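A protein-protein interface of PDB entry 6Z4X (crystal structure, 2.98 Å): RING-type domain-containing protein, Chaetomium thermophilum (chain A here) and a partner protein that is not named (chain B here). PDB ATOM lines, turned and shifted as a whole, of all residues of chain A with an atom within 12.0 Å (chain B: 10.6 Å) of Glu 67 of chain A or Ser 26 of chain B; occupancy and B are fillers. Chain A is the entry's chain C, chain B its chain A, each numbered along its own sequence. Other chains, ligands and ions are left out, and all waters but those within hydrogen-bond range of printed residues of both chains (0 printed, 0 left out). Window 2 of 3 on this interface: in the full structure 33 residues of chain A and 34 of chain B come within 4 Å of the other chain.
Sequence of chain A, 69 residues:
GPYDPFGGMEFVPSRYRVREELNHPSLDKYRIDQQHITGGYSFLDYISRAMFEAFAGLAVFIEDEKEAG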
ATOM      1  N   VAL A  60     -16.636 -24.741 -31.391  1.00  0.00           N
ATOM      2  CA  VAL A  60     -15.617 -25.705 -30.989  1.00  0.00           C
ATOM      3  C   VAL A  60     -14.508 -24.923 -30.290  1.00  0.00           C
ATOM      4  O   VAL A  60     -13.680 -24.280 -30.935  1.00  0.00           O
ATOM      5  CB  VAL A  60     -15.086 -26.503 -32.180  1.00  0.00           C
ATOM      6  CG1 VAL A  60     -13.874 -27.327 -31.767  1.00  0.00           C
ATOM      7  CG2 VAL A  60     -16.176 -27.403 -32.740  1.00  0.00           C
ATOM      8  N   PHE A  61     -14.495 -24.983 -28.961  1.00  0.00           N
ATOM      9  CA  PHE A  61     -13.522 -24.257 -28.147  1.00  0.00           C
ATOM     10  C   PHE A  61     -12.337 -25.180 -27.890  1.00  0.00           C
ATOM     11  O   PHE A  61     -12.373 -26.025 -26.992  1.00  0.00           O
ATOM     12  CB  PHE A  61     -14.173 -23.777 -26.856  1.00  0.00           C
ATOM     13  CG  PHE A  61     -15.495 -23.103 -27.075  1.00  0.00           C
ATOM     14  CD1 PHE A  61     -15.582 -21.959 -27.850  1.00  0.00           C
ATOM     15  CD2 PHE A  61     -16.656 -23.631 -26.536  1.00  0.00           C
ATOM     16  CE1 PHE A  61     -16.799 -21.341 -28.066  1.00  0.00           C
ATOM     17  CE2 PHE A  61     -17.877 -23.017 -26.748  1.00  0.00           C
ATOM     18  CZ  PHE A  61     -17.949 -21.871 -27.515  1.00  0.00           C
ATOM     19  N   ILE A  62     -11.275 -25.007 -28.681  1.00  0.00           N
ATOM     20  CA  ILE A  62     -10.178 -25.971 -28.686  1.00  0.00           C
ATOM     21  C   ILE A  62      -9.514 -26.043 -27.316  1.00  0.00           C
ATOM     22  O   ILE A  62      -9.293 -27.131 -26.770  1.00  0.00           O
ATOM     23  CB  ILE A  62      -9.160 -25.617 -29.785  1.00  0.00           C
ATOM     24  CG1 ILE A  62      -9.763 -25.863 -31.169  1.00  0.00           C
ATOM     25  CG2 ILE A  62      -7.881 -26.421 -29.605  1.00  0.00           C
ATOM     26  CD1 ILE A  62      -8.841 -25.509 -32.319  1.00  0.00           C
ATOM     27  N   GLU A  63      -9.185 -24.886 -26.739  1.00  0.00           N
ATOM     28  CA  GLU A  63      -8.427 -24.875 -25.490  1.00  0.00           C
ATOM     29  C   GLU A  63      -9.165 -25.627 -24.387  1.00  0.00           C
ATOM     30  O   GLU A  63      -8.620 -26.561 -23.783  1.00  0.00           O
ATOM     31  CB  GLU A  63      -8.141 -23.436 -25.064  1.00  0.00           C
ATOM     32  CG  GLU A  63      -7.431 -23.313 -23.724  1.00  0.00           C
ATOM     33  CD  GLU A  63      -6.977 -21.895 -23.428  1.00  0.00           C
ATOM     34  OE1 GLU A  63      -6.462 -21.657 -22.315  1.00  0.00           O
ATOM     35  OE2 GLU A  63      -7.139 -21.020 -24.304  1.00  0.00           O
ATOM     36  N   ASP A  64     -10.415 -25.239 -24.123  1.00  0.00           N
ATOM     37  CA  ASP A  64     -11.168 -25.829 -23.020  1.00  0.00           C
ATOM     38  C   ASP A  64     -11.472 -27.303 -23.269  1.00  0.00           C
ATOM     39  O   ASP A  64     -11.312 -28.137 -22.369  1.00  0.00           O
ATOM     40  CB  ASP A  64     -12.461 -25.043 -22.807  1.00  0.00           C
ATOM     41  CG  ASP A  64     -12.208 -23.568 -22.555  1.00  0.00           C
ATOM     42  OD1 ASP A  64     -11.374 -23.243 -21.685  1.00  0.00           O
ATOM     43  OD2 ASP A  64     -12.833 -22.734 -23.243  1.00  0.00           O
ATOM     44  N   GLU A  65     -11.904 -27.643 -24.485  1.00  0.00           N
ATOM     45  CA  GLU A  65     -12.255 -29.028 -24.786  1.00  0.00           C
ATOM     46  C   GLU A  65     -11.037 -29.939 -24.704  1.00  0.00           C
ATOM     47  O   GLU A  65     -11.148 -31.094 -24.275  1.00  0.00           O
ATOM     48  CB  GLU A  65     -12.907 -29.111 -26.166  1.00  0.00           C
ATOM     49  CG  GLU A  65     -14.264 -28.422 -26.250  1.00  0.00           C
ATOM     50  CD  GLU A  65     -14.789 -28.323 -27.671  1.00  0.00           C
ATOM     51  OE1 GLU A  65     -15.614 -27.423 -27.937  1.00  0.00           O
ATOM     52  OE2 GLU A  65     -14.374 -29.139 -28.522  1.00  0.00           O
ATOM     53  N   LYS A  66      -9.868 -29.443 -25.112  1.00  0.00           N
ATOM     54  CA  LYS A  66      -8.667 -30.271 -25.082  1.00  0.00           C
ATOM     55  C   LYS A  66      -8.088 -30.380 -23.676  1.00  0.00           C
ATOM     56  O   LYS A  66      -7.555 -31.433 -23.306  1.00  0.00           O
ATOM     57  CB  LYS A  66      -7.625 -29.723 -26.056  1.00  0.00           C
ATOM     58  CG  LYS A  66      -7.952 -30.016 -27.513  1.00  0.00           C
ATOM     59  CD  LYS A  66      -7.945 -31.516 -27.778  1.00  0.00           C
ATOM     60  CE  LYS A  66      -8.300 -31.833 -29.222  1.00  0.00           C
ATOM     61  NZ  LYS A  66      -8.323 -33.301 -29.471  1.00  0.00           N
ATOM     62  N   GLU A  67      -8.172 -29.312 -22.876  1.00  0.00           N
ATOM     63  CA  GLU A  67      -7.716 -29.414 -21.495  1.00  0.00           C
ATOM     64  C   GLU A  67      -8.673 -30.224 -20.631  1.00  0.00           C
ATOM     65  O   GLU A  67      -8.253 -30.756 -19.599  1.00  0.00           O
ATOM     66  CB  GLU A  67      -7.513 -28.027 -20.887  1.00  0.00           C
ATOM     67  CG  GLU A  67      -6.211 -27.358 -21.299  1.00  0.00           C
ATOM     68  CD  GLU A  67      -4.994 -27.996 -20.645  1.00  0.00           C
ATOM     69  OE1 GLU A  67      -4.911 -29.242 -20.627  1.00  0.00           O
ATOM     70  OE2 GLU A  67      -4.125 -27.251 -20.142  1.00  0.00           O
ATOM     71  N   ALA A  68      -9.941 -30.336 -21.030  1.00  0.00           N
ATOM     72  CA  ALA A  68     -10.890 -31.161 -20.296  1.00  0.00           C
ATOM     73  C   ALA A  68     -10.701 -32.651 -20.553  1.00  0.00           C
ATOM     74  O   ALA A  68     -11.257 -33.465 -19.807  1.00  0.00           O
ATOM     75  CB  ALA A  68     -12.326 -30.760 -20.647  1.00  0.00           C
ATOM     76  N   GLY A  69      -9.948 -33.025 -21.582  1.00  0.00           N
ATOM     77  CA  GLY A  69      -9.696 -34.424 -21.879  1.00  0.00           C
ATOM     78  C   GLY A  69      -8.416 -34.953 -21.262  1.00  0.00           C
ATOM     79  O   GLY A  69      -7.320 -34.490 -21.585  1.00  0.00           O
ATOM     80  N   TYR B  18      -8.657 -31.695 -35.863  1.00  0.00           N
ATOM     81  CA  TYR B  18      -9.068 -31.465 -34.481  1.00  0.00           C
ATOM     82  C   TYR B  18      -8.477 -32.508 -33.539  1.00  0.00           C
ATOM     83  O   TYR B  18      -7.985 -32.165 -32.458  1.00  0.00           O
ATOM     84  CB  TYR B  18     -10.593 -31.456 -34.391  1.00  0.00           C
ATOM     85  CG  TYR B  18     -11.135 -31.362 -32.983  1.00  0.00           C
ATOM     86  CD1 TYR B  18     -11.310 -30.131 -32.365  1.00  0.00           C
ATOM     87  CD2 TYR B  18     -11.483 -32.505 -32.276  1.00  0.00           C
ATOM     88  CE1 TYR B  18     -11.809 -30.041 -31.079  1.00  0.00           C
ATOM     89  CE2 TYR B  18     -11.982 -32.427 -30.991  1.00  0.00           C
ATOM     90  CZ  TYR B  18     -12.142 -31.193 -30.398  1.00  0.00           C
ATOM     91  OH  TYR B  18     -12.641 -31.108 -29.118  1.00  0.00           O
ATOM     92  N   SER B  22      -4.794 -30.031 -32.817  1.00  0.00           N
ATOM     93  CA  SER B  22      -5.521 -28.976 -32.113  1.00  0.00           C
ATOM     94  C   SER B  22      -5.335 -29.190 -30.617  1.00  0.00           C
ATOM     95  O   SER B  22      -5.818 -30.185 -30.066  1.00  0.00           O
ATOM     96  CB  SER B  22      -7.004 -28.972 -32.483  1.00  0.00           C
ATOM     97  OG  SER B  22      -7.191 -28.615 -33.842  1.00  0.00           O
ATOM     98  N   PHE B  23      -4.642 -28.259 -29.961  1.00  0.00           N
ATOM     99  CA  PHE B  23      -4.315 -28.380 -28.547  1.00  0.00           C
ATOM    100  C   PHE B  23      -4.556 -27.044 -27.860  1.00  0.00           C
ATOM    101  O   PHE B  23      -4.940 -26.054 -28.491  1.00  0.00           O
ATOM    102  CB  PHE B  23      -2.861 -28.818 -28.333  1.00  0.00           C
ATOM    103  CG  PHE B  23      -2.269 -29.568 -29.491  1.00  0.00           C
ATOM    104  CD1 PHE B  23      -2.430 -30.938 -29.603  1.00  0.00           C
ATOM    105  CD2 PHE B  23      -1.536 -28.901 -30.461  1.00  0.00           C
ATOM    106  CE1 PHE B  23      -1.880 -31.629 -30.664  1.00  0.00           C
ATOM    107  CE2 PHE B  23      -0.984 -29.587 -31.524  1.00  0.00           C
ATOM    108  CZ  PHE B  23      -1.157 -30.953 -31.624  1.00  0.00           C
ATOM    109  N   SER B  24      -4.334 -27.030 -26.551  1.00  0.00           N
ATOM    110  CA  SER B  24      -4.309 -25.809 -25.767  1.00  0.00           C
ATOM    111  C   SER B  24      -2.914 -25.204 -25.793  1.00  0.00           C
ATOM    112  O   SER B  24      -1.926 -25.908 -26.022  1.00  0.00           O
ATOM    113  CB  SER B  24      -4.721 -26.097 -24.325  1.00  0.00           C
ATOM    114  OG  SER B  24      -3.729 -26.856 -23.654  1.00  0.00           O
ATOM    115  N   PRO B  25      -2.798 -23.896 -25.569  1.00  0.00           N
ATOM    116  CA  PRO B  25      -1.461 -23.275 -25.579  1.00  0.00           C
ATOM    117  C   PRO B  25      -0.468 -23.980 -24.670  1.00  0.00           C
ATOM    118  O   PRO B  25       0.702 -24.148 -25.042  1.00  0.00           O
ATOM    119  CB  PRO B  25      -1.747 -21.839 -25.115  1.00  0.00           C
ATOM    120  CG  PRO B  25      -3.166 -21.594 -25.522  1.00  0.00           C
ATOM    121  CD  PRO B  25      -3.872 -22.911 -25.354  1.00  0.00           C
ATOM    122  N   SER B  26      -0.910 -24.412 -23.485  1.00  0.00           N
ATOM    123  CA  SER B  26      -0.011 -25.091 -22.560  1.00  0.00           C
ATOM    124  C   SER B  26       0.463 -26.426 -23.121  1.00  0.00           C
ATOM    125  O   SER B  26       1.648 -26.766 -23.009  1.00  0.00           O
ATOM    126  CB  SER B  26      -0.708 -25.298 -21.215  1.00  0.00           C
ATOM    127  OG  SER B  26      -1.819 -26.170 -21.347  1.00  0.00           O
ATOM    128  N   GLN B  27      -0.443 -27.194 -23.730  1.00  0.00           N
ATOM    129  CA  GLN B  27      -0.048 -28.466 -24.325  1.00  0.00           C
ATOM    130  C   GLN B  27       0.962 -28.261 -25.448  1.00  0.00           C
ATOM    131  O   GLN B  27       1.956 -28.989 -25.541  1.00  0.00           O
ATOM    132  CB  GLN B  27      -1.282 -29.211 -24.837  1.00  0.00           C
ATOM    133  CG  GLN B  27      -2.152 -29.796 -23.736  1.00  0.00           C
ATOM    134  CD  GLN B  27      -3.474 -30.322 -24.259  1.00  0.00           C
ATOM    135  OE1 GLN B  27      -3.791 -30.174 -25.440  1.00  0.00           O
ATOM    136  NE2 GLN B  27      -4.254 -30.946 -23.381  1.00  0.00           N
ATOM    137  N   LEU B  28       0.724 -27.268 -26.308  1.00  0.00           N
ATOM    138  CA  LEU B  28       1.651 -26.997 -27.403  1.00  0.00           C
ATOM    139  C   LEU B  28       3.017 -26.575 -26.877  1.00  0.00           C
ATOM    140  O   LEU B  28       4.054 -27.035 -27.374  1.00  0.00           O
ATOM    141  CB  LEU B  28       1.066 -25.917 -28.314  1.00  0.00           C
ATOM    142  CG  LEU B  28       1.550 -25.830 -29.761  1.00  0.00           C
ATOM    143  CD1 LEU B  28       0.731 -24.806 -30.529  1.00  0.00           C
ATOM    144  CD2 LEU B  28       3.016 -25.469 -29.805  1.00  0.00           C
ATOM    145  N   ALA B  29       3.039 -25.694 -25.874  1.00  0.00           N
ATOM    146  CA  ALA B  29       4.308 -25.267 -25.292  1.00  0.00           C
ATOM    147  C   ALA B  29       5.063 -26.447 -24.695  1.00  0.00           C
ATOM    148  O   ALA B  29       6.274 -26.597 -24.903  1.00  0.00           O
ATOM    149  CB  ALA B  29       4.063 -24.189 -24.235  1.00  0.00           C
ATOM    150  N   SER B  30       4.361 -27.299 -23.940  1.00  0.00           N
ATOM    151  CA  SER B  30       5.014 -28.454 -23.335  1.00  0.00           C
ATOM    152  C   SER B  30       5.547 -29.404 -24.398  1.00  0.00           C
ATOM    153  O   SER B  30       6.643 -29.954 -24.255  1.00  0.00           O
ATOM    154  CB  SER B  30       4.047 -29.180 -22.400  1.00  0.00           C
ATOM    155  OG  SER B  30       4.693 -30.252 -21.734  1.00  0.00           O
ATOM    156  N   MET B  31       4.785 -29.608 -25.475  1.00  0.00           N
ATOM    157  CA  MET B  31       5.244 -30.482 -26.549  1.00  0.00           C
ATOM    158  C   MET B  31       6.509 -29.935 -27.197  1.00  0.00           C
ATOM    159  O   MET B  31       7.469 -30.677 -27.432  1.00  0.00           O
ATOM    160  CB  MET B  31       4.140 -30.665 -27.588  1.00  0.00           C
ATOM    161  CG  MET B  31       2.988 -31.532 -27.119  1.00  0.00           C
ATOM    162  SD  MET B  31       1.815 -31.890 -28.436  1.00  0.00           S
ATOM    163  CE  MET B  31       1.060 -30.278 -28.652  1.00  0.00           C
ATOM    164  N   ARG B  32       6.526 -28.635 -27.504  1.00  0.00           N
ATOM    165  CA  ARG B  32       7.714 -28.056 -28.122  1.00  0.00           C
ATOM    166  C   ARG B  32       8.918 -28.146 -27.193  1.00  0.00           C
ATOM    167  O   ARG B  32      10.028 -28.483 -27.628  1.00  0.00           O
ATOM    168  CB  ARG B  32       7.448 -26.606 -28.527  1.00  0.00           C
ATOM    169  CG  ARG B  32       6.550 -26.463 -29.743  1.00  0.00           C
ATOM    170  CD  ARG B  32       6.230 -25.007 -30.012  1.00  0.00           C
ATOM    171  NE  ARG B  32       5.539 -24.825 -31.285  1.00  0.00           N
ATOM    172  CZ  ARG B  32       4.893 -23.717 -31.631  1.00  0.00           C
ATOM    173  NH1 ARG B  32       4.842 -22.689 -30.795  1.00  0.00           N
ATOM    174  NH2 ARG B  32       4.290 -23.637 -32.808  1.00  0.00           N
ATOM    175  N   GLU B  33       8.715 -27.867 -25.903  1.00  0.00           N
ATOM    176  CA  GLU B  33       9.818 -27.943 -24.951  1.00  0.00           C
ATOM    177  C   GLU B  33      10.349 -29.367 -24.837  1.00  0.00           C
ATOM    178  O   GLU B  33      11.567 -29.582 -24.805  1.00  0.00           O
ATOM    179  CB  GLU B  33       9.362 -27.418 -23.587  1.00  0.00           C
ATOM    180  CG  GLU B  33      10.447 -27.375 -22.513  1.00  0.00           C
ATOM    181  CD  GLU B  33      10.608 -28.689 -21.769  1.00  0.00           C
ATOM    182  OE1 GLU B  33       9.613 -29.437 -21.661  1.00  0.00           O
ATOM    183  OE2 GLU B  33      11.727 -28.964 -21.283  1.00  0.00           O
ATOM    184  N   LYS B  34       9.451 -30.354 -24.785  1.00  0.00           N
ATOM    185  CA  LYS B  34       9.885 -31.742 -24.671  1.00  0.00           C
ATOM    186  C   LYS B  34      10.584 -32.212 -25.941  1.00  0.00           C
ATOM    187  O   LYS B  34      11.548 -32.979 -25.872  1.00  0.00           O
ATOM    188  CB  LYS B  34       8.697 -32.643 -24.336  1.00  0.00           C
ATOM    189  CG  LYS B  34       8.183 -32.467 -22.914  1.00  0.00           C
ATOM    190  CD  LYS B  34       7.002 -33.379 -22.613  1.00  0.00           C
ATOM    191  CE  LYS B  34       6.565 -33.244 -21.157  1.00  0.00           C
ATOM    192  NZ  LYS B  34       5.499 -34.218 -20.785  1.00  0.00           N
ATOM    193  N   ILE B 123       6.801 -29.086 -34.987  1.00  0.00           N
ATOM    194  CA  ILE B 123       6.280 -29.247 -33.638  1.00  0.00           C
ATOM    195  C   ILE B 123       6.477 -30.682 -33.153  1.00  0.00           C
ATOM    196  O   ILE B 123       6.667 -30.902 -31.953  1.00  0.00           O
ATOM    197  CB  ILE B 123       4.802 -28.830 -33.554  1.00  0.00           C
ATOM    198  CG1 ILE B 123       4.272 -29.031 -32.134  1.00  0.00           C
ATOM    199  CG2 ILE B 123       3.965 -29.637 -34.510  1.00  0.00           C
ATOM    200  CD1 ILE B 123       2.868 -28.490 -31.924  1.00  0.00           C
ATOM    201  N   ASP B 229       0.204 -19.288 -34.238  1.00  0.00           N
ATOM    202  CA  ASP B 229      -0.359 -20.583 -33.870  1.00  0.00           C
ATOM    203  C   ASP B 229      -1.877 -20.628 -34.014  1.00  0.00           C
ATOM    204  O   ASP B 229      -2.549 -21.311 -33.231  1.00  0.00           O
ATOM    205  CB  ASP B 229       0.059 -20.949 -32.446  1.00  0.00           C
ATOM    206  CG  ASP B 229       1.564 -21.054 -32.291  1.00  0.00           C
ATOM    207  OD1 ASP B 229       2.259 -21.193 -33.318  1.00  0.00           O
ATOM    208  OD2 ASP B 229       2.051 -20.997 -31.143  1.00  0.00           O
ATOM    209  N   PHE B 232      -3.657 -24.017 -34.443  1.00  0.00           N
ATOM    210  CA  PHE B 232      -3.556 -24.952 -33.330  1.00  0.00           C
ATOM    211  C   PHE B 232      -4.600 -24.722 -32.244  1.00  0.00           C
ATOM    212  O   PHE B 232      -4.917 -25.660 -31.506  1.00  0.00           O
ATOM    213  CB  PHE B 232      -2.154 -24.890 -32.720  1.00  0.00           C
ATOM    214  CG  PHE B 232      -1.063 -25.242 -33.689  1.00  0.00           C
ATOM    215  CD1 PHE B 232      -0.962 -26.527 -34.199  1.00  0.00           C
ATOM    216  CD2 PHE B 232      -0.143 -24.292 -34.095  1.00  0.00           C
ATOM    217  CE1 PHE B 232       0.038 -26.857 -35.093  1.00  0.00           C
ATOM    218  CE2 PHE B 232       0.858 -24.616 -34.990  1.00  0.00           C
ATOM    219  CZ  PHE B 232       0.949 -25.901 -35.489  1.00  0.00           C
ATOM    220  N   HIS B 233      -5.140 -23.509 -32.125  1.00  0.00           N
ATOM    221  CA  HIS B 233      -6.070 -23.189 -31.052  1.00  0.00           C
ATOM    222  C   HIS B 233      -7.446 -22.750 -31.526  1.00  0.00           C
ATOM    223  O   HIS B 233      -8.333 -22.558 -30.685  1.00  0.00           O
ATOM    224  CB  HIS B 233      -5.491 -22.091 -30.146  1.00  0.00           C
ATOM    225  CG  HIS B 233      -4.080 -22.341 -29.719  1.00  0.00           C
ATOM    226  ND1 HIS B 233      -3.702 -23.473 -29.031  1.00  0.00           N
ATOM    227  CD2 HIS B 233      -2.956 -21.603 -29.876  1.00  0.00           C
ATOM    228  CE1 HIS B 233      -2.404 -23.425 -28.786  1.00  0.00           C
ATOM    229  NE2 HIS B 233      -1.929 -22.300 -29.289  1.00  0.00           N
ATOM    230  N   LYS B 317     -19.156 -17.034 -25.333  1.00  0.00           N
ATOM    231  CA  LYS B 317     -17.938 -17.831 -25.462  1.00  0.00           C
ATOM    232  C   LYS B 317     -17.370 -17.742 -26.875  1.00  0.00           C
ATOM    233  O   LYS B 317     -16.149 -17.646 -27.058  1.00  0.00           O
ATOM    234  CB  LYS B 317     -18.222 -19.286 -25.080  1.00  0.00           C
ATOM    235  CG  LYS B 317     -16.978 -20.123 -24.822  1.00  0.00           C
ATOM    236  CD  LYS B 317     -16.203 -19.607 -23.615  1.00  0.00           C
ATOM    237  CE  LYS B 317     -15.028 -20.513 -23.279  1.00  0.00           C
ATOM    238  NZ  LYS B 317     -13.971 -20.483 -24.329  1.00  0.00           N
ATOM    239  N   MET B 328      -4.323 -12.669 -31.403  1.00  0.00           N
ATOM    240  CA  MET B 328      -3.210 -13.490 -31.870  1.00  0.00           C
ATOM    241  C   MET B 328      -2.855 -13.153 -33.312  1.00  0.00           C
ATOM    242  O   MET B 328      -1.676 -13.150 -33.684  1.00  0.00           O
ATOM    243  CB  MET B 328      -3.543 -14.976 -31.733  1.00  0.00           C
ATOM    244  CG  MET B 328      -2.416 -15.897 -32.184  1.00  0.00           C
ATOM    245  SD  MET B 328      -2.718 -17.643 -31.847  1.00  0.00           S
ATOM    246  CE  MET B 328      -2.811 -17.631 -30.059  1.00  0.00           C
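OE2 of Glu 65 of chain A is in hydrogen-bond range of OH of Tyr 18 of chain B, at 2.7 Å.
The backbone carbonyl oxygen (O) of Tyr 18 of chain B sits at hydrogen-bond distance from the side-chain amino group (NZ) of Lys 66 of chain A, 3.2 Å away.
The side-chain hydroxyl (OG) of Ser 26 of chain B is in hydrogen-bond range of the side-chain carboxylate (OE2) of Glu 67 of chain A.
The side-chain amide nitrogen of Gln 27 of chain B sits at hydrogen-bond distance from the backbone carbonyl oxygen of Lys 66 of chain A, at 3.3 Å.
NE2 of Gln 27 of chain B sits at hydrogen-bond distance from OE1 of Glu 67 of chain A (3.3 Å).
The side-chain amino group (NZ) of Lys 317 of chain B is in salt-bridge range of the side-chain carboxylate (OD2) of Asp 64 of chain A (2.7 Å).
The backbone NH (N) of Phe 23 of chain B sits at hydrogen-bond distance from the backbone carbonyl oxygen (O) of Phe 232 of chain B, at 3.0 Å.
The backbone carbonyl oxygen (O) of Phe 23 of chain B is in hydrogen-bond range of a ring nitrogen (ND1) of His 233 of chain B, at 2.9 Å.
OG of Ser 24 of chain B sits at hydrogen-bond distance from OG of Ser 26 of chain B (3.1 Å).
The backbone NH (N) of Gln 27 of chain B is in hydrogen-bond range of the side-chain hydroxyl (OG) of Ser 24 of chain B (3.3 Å).
N of Phe 61 of chain A is in hydrogen-bond range of OE1 of Glu 65 of chain A (2.9 Å).
Among the printed residues, merely in contact across the chains: Val 60 of chain A with Tyr 18 of chain B, Phe 61 of chain A with Lys 317 of chain B, Ile 62 of chain A with Ser 22 of chain B, Ile 62 of chain A with Phe 23 of chain B, Ile 62 of chain A with Phe 232 of chain B, Ile 62 of chain A with His 233 of chain B, Glu 63 of chain A with Ser 24 of chain B, Glu 63 of chain A with Pro 25 of chain B, Lys 66 of chain A with Ser 22 of chain B and Glu 67 of chain A with Ser 24 of chain B.
Glu 67 of chain A touches just these residues of chain B: Ser 24 (3.5 Å), Ser 26 (2.8 Å) and Gln 27 (3.3 Å).
Ser 26 of chain B touches just one residue of chain A: Glu 67.
No residue of chain B comes within 4 Å of Ala 68 of chain A.
Pro 25 of chain B touches just one residue of chain A: Glu 63 (3.8 Å).
Of chain A, only Lys 66 (3.3 Å) and Glu 67 (3.3 Å) come within 4 Å of Gln 27 of chain B.
Leu 28 of chain B touches none of the printed residues of chain A.
No residue of chain A comes within 4 Å of Ala 29 of chain B.
No residue of chain A comes within 4 Å of Ser 30 of chain B.
Of the printed residues of chain A, Lys 317 of chain B touches Phe 61 (3.4 Å) and Asp 64 (2.7 Å).
Of the printed residues of chain A, Phe 23 of chain B touches Ile 62 (3.2 Å).
Printed residues of chain A within 4 Å of Tyr 18 of chain B: Val 60 (3.5 Å), Glu 65 (2.7 Å) and Lys 66 (3.2 Å).
Printed residues of chain B within 4 Å of Lys 66 of chain A: Tyr 18, Ser 22 and Gln 27.
Lys 34 of chain B touches none of the printed residues of chain A.
Hydrophobic or aromatic side chains of chain B that line the printed part of chain A: Tyr 18 and Pro 25.
Printed residues of chain A that touch a printed residue of chain B: Val 60, Phe 61, Ile 62, Glu 63, Asp 64, Glu 65, Lys 66 and Glu 67.
Hydrophobic or aromatic side chains of chain A within 4 Å of the printed part of chain B: Val 60, Phe 61 and Ile 62.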
